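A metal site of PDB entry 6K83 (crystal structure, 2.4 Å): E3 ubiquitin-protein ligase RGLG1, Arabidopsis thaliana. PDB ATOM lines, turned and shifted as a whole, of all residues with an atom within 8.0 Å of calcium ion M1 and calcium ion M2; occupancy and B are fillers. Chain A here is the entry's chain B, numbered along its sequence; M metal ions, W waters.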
ATOM      1  N   SER A  13     -29.807 -10.093  16.637  1.00  0.00           N
ATOM      2  CA  SER A  13     -31.157 -10.538  16.945  1.00  0.00           C
ATOM      3  C   SER A  13     -31.149 -11.428  18.185  1.00  0.00           C
ATOM      4  O   SER A  13     -30.089 -11.666  18.764  1.00  0.00           O
ATOM      5  CB  SER A  13     -31.767 -11.293  15.742  1.00  0.00           C
ATOM      6  OG  SER A  13     -32.965 -11.975  16.085  1.00  0.00           O
ATOM      7  N   LYS A  14     -32.321 -11.913  18.588  1.00  0.00           N
ATOM      8  CA  LYS A  14     -32.458 -12.859  19.688  1.00  0.00           C
ATOM      9  C   LYS A  14     -32.583 -14.300  19.172  1.00  0.00           C
ATOM     10  O   LYS A  14     -33.409 -14.585  18.295  1.00  0.00           O
ATOM     11  CB  LYS A  14     -33.664 -12.501  20.536  1.00  0.00           C
ATOM     12  CG  LYS A  14     -34.117 -13.628  21.457  1.00  0.00           C
ATOM     13  CD  LYS A  14     -35.428 -13.263  22.142  1.00  0.00           C
ATOM     14  CE  LYS A  14     -36.268 -14.498  22.379  1.00  0.00           C
ATOM     15  NZ  LYS A  14     -35.412 -15.741  22.350  1.00  0.00           N
ATOM     16  N   ILE A  15     -31.774 -15.192  19.741  1.00  0.00           N
ATOM     17  CA  ILE A  15     -31.686 -16.603  19.338  1.00  0.00           C
ATOM     18  C   ILE A  15     -32.671 -17.523  20.080  1.00  0.00           C
ATOM     19  O   ILE A  15     -32.582 -17.731  21.302  1.00  0.00           O
ATOM     20  CB  ILE A  15     -30.253 -17.142  19.582  1.00  0.00           C
ATOM     21  CG1 ILE A  15     -29.227 -16.335  18.780  1.00  0.00           C
ATOM     22  CG2 ILE A  15     -30.165 -18.632  19.242  1.00  0.00           C
ATOM     23  CD1 ILE A  15     -27.786 -16.484  19.279  1.00  0.00           C
ATOM     24  N   SER A  16     -33.607 -18.077  19.318  1.00  0.00           N
ATOM     25  CA  SER A  16     -34.542 -19.052  19.861  1.00  0.00           C
ATOM     26  C   SER A  16     -33.876 -20.423  19.987  1.00  0.00           C
ATOM     27  O   SER A  16     -32.780 -20.636  19.462  1.00  0.00           O
ATOM     28  CB  SER A  16     -35.792 -19.154  18.981  1.00  0.00           C
ATOM     29  OG  SER A  16     -36.760 -18.181  19.356  1.00  0.00           O
ATOM     30  N   ASP A  17     -34.543 -21.325  20.691  1.00  0.00           N
ATOM     31  CA  ASP A  17     -34.132 -22.722  20.722  1.00  0.00           C
ATOM     32  C   ASP A  17     -34.388 -23.355  19.358  1.00  0.00           C
ATOM     33  O   ASP A  17     -35.535 -23.556  18.963  1.00  0.00           O
ATOM     34  CB  ASP A  17     -34.882 -23.468  21.829  1.00  0.00           C
ATOM     35  CG  ASP A  17     -34.659 -22.862  23.192  1.00  0.00           C
ATOM     36  OD1 ASP A  17     -34.071 -21.751  23.261  1.00  0.00           O
ATOM     37  OD2 ASP A  17     -35.067 -23.464  24.198  1.00  0.00           O
ATOM     38  N   ILE A 203     -21.724 -16.537  26.601  1.00  0.00           N
ATOM     39  CA  ILE A 203     -21.941 -16.627  28.037  1.00  0.00           C
ATOM     40  C   ILE A 203     -23.036 -17.649  28.302  1.00  0.00           C
ATOM     41  O   ILE A 203     -24.055 -17.657  27.628  1.00  0.00           O
ATOM     42  CB  ILE A 203     -22.306 -15.255  28.657  1.00  0.00           C
ATOM     43  CG1 ILE A 203     -21.259 -14.207  28.255  1.00  0.00           C
ATOM     44  CG2 ILE A 203     -22.389 -15.353  30.180  1.00  0.00           C
ATOM     45  CD1 ILE A 203     -21.620 -12.778  28.589  1.00  0.00           C
ATOM     46  N   MET A 216     -32.482 -13.411  34.855  1.00  0.00           N
ATOM     47  CA  MET A 216     -31.622 -14.225  34.014  1.00  0.00           C
ATOM     48  C   MET A 216     -32.267 -14.386  32.657  1.00  0.00           C
ATOM     49  O   MET A 216     -31.588 -14.293  31.653  1.00  0.00           O
ATOM     50  CB  MET A 216     -31.345 -15.563  34.681  1.00  0.00           C
ATOM     51  CG  MET A 216     -30.635 -15.458  36.043  1.00  0.00           C
ATOM     52  SD  MET A 216     -29.030 -14.627  35.969  1.00  0.00           S
ATOM     53  CE  MET A 216     -29.473 -12.940  36.405  1.00  0.00           C
ATOM     54  N   GLN A 217     -33.589 -14.585  32.627  1.00  0.00           N
ATOM     55  CA  GLN A 217     -34.314 -14.676  31.364  1.00  0.00           C
ATOM     56  C   GLN A 217     -34.221 -13.367  30.574  1.00  0.00           C
ATOM     57  O   GLN A 217     -34.214 -13.405  29.350  1.00  0.00           O
ATOM     58  CB  GLN A 217     -35.766 -15.066  31.595  1.00  0.00           C
ATOM     59  CG  GLN A 217     -35.981 -16.528  31.937  1.00  0.00           C
ATOM     60  CD  GLN A 217     -37.177 -16.754  32.866  1.00  0.00           C
ATOM     61  OE1 GLN A 217     -37.740 -15.815  33.437  1.00  0.00           O
ATOM     62  NE2 GLN A 217     -37.559 -18.014  33.034  1.00  0.00           N
ATOM     63  N   GLU A 218     -34.151 -12.226  31.270  1.00  0.00           N
ATOM     64  CA  GLU A 218     -33.959 -10.938  30.599  1.00  0.00           C
ATOM     65  C   GLU A 218     -32.581 -10.879  29.937  1.00  0.00           C
ATOM     66  O   GLU A 218     -32.449 -10.409  28.802  1.00  0.00           O
ATOM     67  CB  GLU A 218     -34.111  -9.749  31.562  1.00  0.00           C
ATOM     68  CG  GLU A 218     -35.542  -9.286  31.790  1.00  0.00           C
ATOM     69  CD  GLU A 218     -36.199  -8.669  30.551  1.00  0.00           C
ATOM     70  OE1 GLU A 218     -35.579  -7.801  29.907  1.00  0.00           O
ATOM     71  OE2 GLU A 218     -37.334  -9.072  30.231  1.00  0.00           O
ATOM     72  N   PHE A 219     -31.564 -11.341  30.660  1.00  0.00           N
ATOM     73  CA  PHE A 219     -30.211 -11.376  30.120  1.00  0.00           C
ATOM     74  C   PHE A 219     -30.178 -12.310  28.904  1.00  0.00           C
ATOM     75  O   PHE A 219     -29.499 -12.008  27.918  1.00  0.00           O
ATOM     76  CB  PHE A 219     -29.186 -11.800  31.179  1.00  0.00           C
ATOM     77  CG  PHE A 219     -29.001 -10.772  32.290  1.00  0.00           C
ATOM     78  CD1 PHE A 219     -29.591  -9.513  32.205  1.00  0.00           C
ATOM     79  CD2 PHE A 219     -28.242 -11.057  33.413  1.00  0.00           C
ATOM     80  CE1 PHE A 219     -29.427  -8.576  33.208  1.00  0.00           C
ATOM     81  CE2 PHE A 219     -28.075 -10.115  34.423  1.00  0.00           C
ATOM     82  CZ  PHE A 219     -28.663  -8.880  34.315  1.00  0.00           C
ATOM     83  N   ASP A 220     -30.936 -13.408  28.959  1.00  0.00           N
ATOM     84  CA  ASP A 220     -30.959 -14.399  27.875  1.00  0.00           C
ATOM     85  C   ASP A 220     -31.584 -13.785  26.609  1.00  0.00           C
ATOM     86  O   ASP A 220     -30.992 -13.818  25.535  1.00  0.00           O
ATOM     87  CB  ASP A 220     -31.751 -15.651  28.316  1.00  0.00           C
ATOM     88  CG  ASP A 220     -31.708 -16.830  27.280  1.00  0.00           C
ATOM     89  OD1 ASP A 220     -31.140 -16.681  26.188  1.00  0.00           O
ATOM     90  OD2 ASP A 220     -32.271 -17.924  27.559  1.00  0.00           O
ATOM     91  N   ASP A 221     -32.755 -13.171  26.770  1.00  0.00           N
ATOM     92  CA  ASP A 221     -33.600 -12.804  25.643  1.00  0.00           C
ATOM     93  C   ASP A 221     -33.698 -11.333  25.277  1.00  0.00           C
ATOM     94  O   ASP A 221     -33.965 -11.014  24.115  1.00  0.00           O
ATOM     95  CB  ASP A 221     -35.015 -13.326  25.911  1.00  0.00           C
ATOM     96  CG  ASP A 221     -35.094 -14.832  25.844  1.00  0.00           C
ATOM     97  OD1 ASP A 221     -34.437 -15.416  24.957  1.00  0.00           O
ATOM     98  OD2 ASP A 221     -35.797 -15.431  26.687  1.00  0.00           O
ATOM     99  N   ASN A 222     -33.515 -10.430  26.242  1.00  0.00           N
ATOM    100  CA  ASN A 222     -33.818  -9.014  25.982  1.00  0.00           C
ATOM    101  C   ASN A 222     -32.746  -8.013  26.401  1.00  0.00           C
ATOM    102  O   ASN A 222     -32.895  -7.310  27.428  1.00  0.00           O
ATOM    103  CB  ASN A 222     -35.135  -8.643  26.664  1.00  0.00           C
ATOM    104  CG  ASN A 222     -35.607  -7.232  26.318  1.00  0.00           C
ATOM    105  OD1 ASN A 222     -35.912  -6.957  25.159  1.00  0.00           O
ATOM    106  ND2 ASN A 222     -35.645  -6.343  27.309  1.00  0.00           N
ATOM    107  N   ARG A 226     -26.876  -4.779  22.670  1.00  0.00           N
ATOM    108  CA  ARG A 226     -25.731  -5.645  22.351  1.00  0.00           C
ATOM    109  C   ARG A 226     -25.731  -6.053  20.881  1.00  0.00           C
ATOM    110  O   ARG A 226     -26.783  -6.043  20.238  1.00  0.00           O
ATOM    111  CB  ARG A 226     -25.706  -6.888  23.237  1.00  0.00           C
ATOM    112  CG  ARG A 226     -26.787  -7.914  22.939  1.00  0.00           C
ATOM    113  CD  ARG A 226     -26.740  -9.098  23.921  1.00  0.00           C
ATOM    114  NE  ARG A 226     -28.026  -9.779  23.992  1.00  0.00           N
ATOM    115  CZ  ARG A 226     -28.358 -10.688  24.917  1.00  0.00           C
ATOM    116  NH1 ARG A 226     -27.485 -11.050  25.859  1.00  0.00           N
ATOM    117  NH2 ARG A 226     -29.571 -11.234  24.890  1.00  0.00           N
ATOM    118  N   PHE A 228     -24.853  -8.936  19.426  1.00  0.00           N
ATOM    119  CA  PHE A 228     -25.474 -10.222  19.142  1.00  0.00           C
ATOM    120  C   PHE A 228     -25.887 -10.866  20.436  1.00  0.00           C
ATOM    121  O   PHE A 228     -25.444 -10.460  21.518  1.00  0.00           O
ATOM    122  CB  PHE A 228     -24.524 -11.143  18.330  1.00  0.00           C
ATOM    123  CG  PHE A 228     -23.344 -11.668  19.104  1.00  0.00           C
ATOM    124  CD1 PHE A 228     -22.132 -10.998  19.100  1.00  0.00           C
ATOM    125  CD2 PHE A 228     -23.433 -12.859  19.819  1.00  0.00           C
ATOM    126  CE1 PHE A 228     -21.021 -11.506  19.803  1.00  0.00           C
ATOM    127  CE2 PHE A 228     -22.345 -13.363  20.514  1.00  0.00           C
ATOM    128  CZ  PHE A 228     -21.129 -12.686  20.516  1.00  0.00           C
ATOM    129  N   ASP A 229     -26.742 -11.869  20.325  1.00  0.00           N
ATOM    130  CA  ASP A 229     -27.241 -12.595  21.475  1.00  0.00           C
ATOM    131  C   ASP A 229     -26.135 -13.499  22.033  1.00  0.00           C
ATOM    132  O   ASP A 229     -25.871 -14.589  21.486  1.00  0.00           O
ATOM    133  CB  ASP A 229     -28.479 -13.401  21.069  1.00  0.00           C
ATOM    134  CG  ASP A 229     -29.222 -13.971  22.253  1.00  0.00           C
ATOM    135  OD1 ASP A 229     -28.715 -13.849  23.390  1.00  0.00           O
ATOM    136  OD2 ASP A 229     -30.308 -14.532  22.035  1.00  0.00           O
ATOM    137  N   ASN A 230     -25.481 -13.025  23.100  1.00  0.00           N
ATOM    138  CA  ASN A 230     -24.299 -13.722  23.637  1.00  0.00           C
ATOM    139  C   ASN A 230     -24.570 -14.394  24.973  1.00  0.00           C
ATOM    140  O   ASN A 230     -23.640 -14.862  25.612  1.00  0.00           O
ATOM    141  CB  ASN A 230     -23.132 -12.751  23.809  1.00  0.00           C
ATOM    142  CG  ASN A 230     -23.482 -11.568  24.702  1.00  0.00           C
ATOM    143  OD1 ASN A 230     -24.604 -11.467  25.217  1.00  0.00           O
ATOM    144  ND2 ASN A 230     -22.530 -10.649  24.874  1.00  0.00           N
ATOM    145  N   PHE A 231     -25.820 -14.436  25.398  1.00  0.00           N
ATOM    146  CA  PHE A 231     -26.129 -14.931  26.728  1.00  0.00           C
ATOM    147  C   PHE A 231     -27.190 -16.007  26.667  1.00  0.00           C
ATOM    148  O   PHE A 231     -28.250 -15.793  26.095  1.00  0.00           O
ATOM    149  CB  PHE A 231     -26.596 -13.771  27.602  1.00  0.00           C
ATOM    150  CG  PHE A 231     -26.541 -14.044  29.089  1.00  0.00           C
ATOM    151  CD1 PHE A 231     -27.507 -14.819  29.705  1.00  0.00           C
ATOM    152  CD2 PHE A 231     -25.548 -13.471  29.876  1.00  0.00           C
ATOM    153  CE1 PHE A 231     -27.489 -15.033  31.048  1.00  0.00           C
ATOM    154  CE2 PHE A 231     -25.515 -13.682  31.253  1.00  0.00           C
ATOM    155  CZ  PHE A 231     -26.490 -14.468  31.838  1.00  0.00           C
ATOM    156  N   GLN A 232     -26.901 -17.162  27.263  1.00  0.00           N
ATOM    157  CA  GLN A 232     -27.893 -18.237  27.405  1.00  0.00           C
ATOM    158  C   GLN A 232     -28.164 -18.572  28.888  1.00  0.00           C
ATOM    159  O   GLN A 232     -27.257 -18.512  29.721  1.00  0.00           O
ATOM    160  CB  GLN A 232     -27.448 -19.504  26.651  1.00  0.00           C
ATOM    161  CG  GLN A 232     -28.210 -20.812  26.995  1.00  0.00           C
ATOM    162  CD  GLN A 232     -29.691 -20.792  26.557  1.00  0.00           C
ATOM    163  OE1 GLN A 232     -30.314 -19.747  26.492  1.00  0.00           O
ATOM    164  NE2 GLN A 232     -30.249 -21.966  26.278  1.00  0.00           N
ATOM    165  N   PHE A 233     -29.419 -18.902  29.210  1.00  0.00           N
ATOM    166  CA  PHE A 233     -29.806 -19.228  30.580  1.00  0.00           C
ATOM    167  C   PHE A 233     -30.232 -20.689  30.730  1.00  0.00           C
ATOM    168  O   PHE A 233     -31.080 -21.182  29.998  1.00  0.00           O
ATOM    169  CB  PHE A 233     -30.949 -18.312  31.061  1.00  0.00           C
ATOM    170  CG  PHE A 233     -31.589 -18.777  32.356  1.00  0.00           C
ATOM    171  CD1 PHE A 233     -30.808 -19.024  33.489  1.00  0.00           C
ATOM    172  CD2 PHE A 233     -32.955 -18.948  32.442  1.00  0.00           C
ATOM    173  CE1 PHE A 233     -31.397 -19.469  34.692  1.00  0.00           C
ATOM    174  CE2 PHE A 233     -33.543 -19.384  33.636  1.00  0.00           C
ATOM    175  CZ  PHE A 233     -32.760 -19.644  34.766  1.00  0.00           C
ATOM    176  N   VAL A 234     -29.635 -21.361  31.707  1.00  0.00           N
ATOM    177  CA  VAL A 234     -29.973 -22.742  31.973  1.00  0.00           C
ATOM    178  C   VAL A 234     -30.536 -22.827  33.377  1.00  0.00           C
ATOM    179  O   VAL A 234     -29.866 -22.435  34.321  1.00  0.00           O
ATOM    180  CB  VAL A 234     -28.722 -23.661  31.831  1.00  0.00           C
ATOM    181  CG1 VAL A 234     -29.108 -25.134  31.927  1.00  0.00           C
ATOM    182  CG2 VAL A 234     -28.011 -23.357  30.523  1.00  0.00           C
ATOM    183  N   SER A 256     -29.336 -27.786  26.545  1.00  0.00           N
ATOM    184  CA  SER A 256     -29.703 -26.475  27.030  1.00  0.00           C
ATOM    185  C   SER A 256     -28.466 -25.561  27.071  1.00  0.00           C
ATOM    186  O   SER A 256     -28.527 -24.407  26.640  1.00  0.00           O
ATOM    187  CB  SER A 256     -30.367 -26.583  28.390  1.00  0.00           C
ATOM    188  OG  SER A 256     -31.056 -25.390  28.666  1.00  0.00           O
ATOM    189  N   MET A 259     -27.339 -24.691  23.333  1.00  0.00           N
ATOM    190  CA  MET A 259     -28.411 -24.314  22.437  1.00  0.00           C
ATOM    191  C   MET A 259     -28.103 -23.092  21.575  1.00  0.00           C
ATOM    192  O   MET A 259     -28.561 -22.998  20.421  1.00  0.00           O
ATOM    193  CB  MET A 259     -29.691 -24.065  23.252  1.00  0.00           C
ATOM    194  CG  MET A 259     -30.918 -23.735  22.427  1.00  0.00           C
ATOM    195  SD  MET A 259     -31.597 -25.170  21.581  1.00  0.00           S
ATOM    196  CE  MET A 259     -32.276 -26.083  22.969  1.00  0.00           C
ATOM    197  N   GLU A 260     -27.306 -22.174  22.103  1.00  0.00           N
ATOM    198  CA  GLU A 260     -27.003 -20.928  21.370  1.00  0.00           C
ATOM    199  C   GLU A 260     -25.567 -20.885  20.845  1.00  0.00           C
ATOM    200  O   GLU A 260     -25.162 -19.915  20.199  1.00  0.00           O
ATOM    201  CB  GLU A 260     -27.272 -19.708  22.259  1.00  0.00           C
ATOM    202  CG  GLU A 260     -28.734 -19.554  22.691  1.00  0.00           C
ATOM    203  CD  GLU A 260     -29.030 -18.186  23.325  1.00  0.00           C
ATOM    204  OE1 GLU A 260     -28.228 -17.236  23.168  1.00  0.00           O
ATOM    205  OE2 GLU A 260     -30.085 -18.059  23.990  1.00  0.00           O
ATOM    206  N   GLN A 264     -24.047 -18.295  17.926  1.00  0.00           N
ATOM    207  CA  GLN A 264     -23.151 -17.309  18.531  1.00  0.00           C
ATOM    208  C   GLN A 264     -21.741 -17.409  17.967  1.00  0.00           C
ATOM    209  O   GLN A 264     -21.027 -16.400  17.843  1.00  0.00           O
ATOM    210  CB  GLN A 264     -23.111 -17.485  20.037  1.00  0.00           C
ATOM    211  CG  GLN A 264     -24.381 -17.027  20.727  1.00  0.00           C
ATOM    212  CD  GLN A 264     -24.386 -17.413  22.179  1.00  0.00           C
ATOM    213  OE1 GLN A 264     -23.555 -18.208  22.608  1.00  0.00           O
ATOM    214  NE2 GLN A 264     -25.328 -16.863  22.950  1.00  0.00           N
HETATM  215 CA    CA M   1     -32.038 -18.700  25.335  1.00  0.00          CA
HETATM  216 CA    CA M   2     -29.952 -15.747  24.355  1.00  0.00          CA
HETATM  217  O   HOH W   1     -32.835 -20.471  26.708  1.00  0.00           O
HETATM  218  O   HOH W   2     -32.420 -16.186  23.680  1.00  0.00           O
HETATM  219  O   HOH W   3     -34.224 -18.043  25.391  1.00  0.00           O
HETATM  220  O   HOH W   4     -32.750 -19.978  23.014  1.00  0.00           O
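The backbone carbonyl oxygen (O) of Glu 260 sits close to the side-chain amide oxygen (OE1) of Gln 264 (3.4 Å). The side-chain carboxylate (OD1) of Asp 229 sits close to the guanidinium group (NH2) of Arg 226, at 3.1 Å. The backbone carbonyl oxygen of Ser 256 sits at hydrogen-bond distance from the side-chain amide nitrogen of Gln 232, 3.0 Å away. The side-chain amide nitrogen (NE2) of Gln 264 is in hydrogen-bond range of the backbone carbonyl oxygen (O) of Asp 229 (2.8 Å). O of Asp 220 sits close to NH2 of Arg 226 (3.0 Å). OD2 of Asp 220 sits close to N of Phe 233 (3.4 Å). The backbone NH of Ile 15 lies close to the side-chain carboxylate of Asp 229 (2.8 Å). N of Gln 232 lies within hydrogen-bond range of O of Ile 203, 2.9 Å away.
Along chain A the residues within 4 Å of calcium ion M1 span positions 220 to 260.
Four residues have an atom within 4 Å of calcium ion M2: Asp 220, Asp 229, Phe 231 and Glu 260. The nearest printed residue that does not touch calcium ion M2 is Gln 232 (4.4 Å).
Calcium ion M1 is bound by water W3, OE1 of Gln 232, OD2 of Asp 220, OD1 of Asp 220, water W1, OE2 of Glu 260 and water W4. Calcium ion M1 has seven donor atoms within binding distance. Slightly farther from calcium ion M1 lies water W2 (3.0 Å).
Calcium ion M2 is bound by OE2 of Glu 260. OD1 of Asp 220 is bound to calcium ion M2. Calcium ion M2 is bound by O of Phe 231, 2.4 Å away. The side-chain carboxylate (OD1) of Asp 229 binds calcium ion M2 (2.5 Å). The backbone carbonyl oxygen (O) of Asp 220 binds calcium ion M2 (2.5 Å). OE1 of Glu 260 is bound to calcium ion M2. Calcium ion M2 is bound by water W2, at 2.6 Å. Calcium ion M2 is bound by OD2 of Asp 229, 2.6 Å away. Calcium ion M2 has eight donor atoms within binding distance.
Water W2 lies within hydrogen-bond range of OD1 of Asp 221 (2.5 Å), O of Ile 15 (2.8 Å) and NZ of Lys 14 (3.3 Å).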
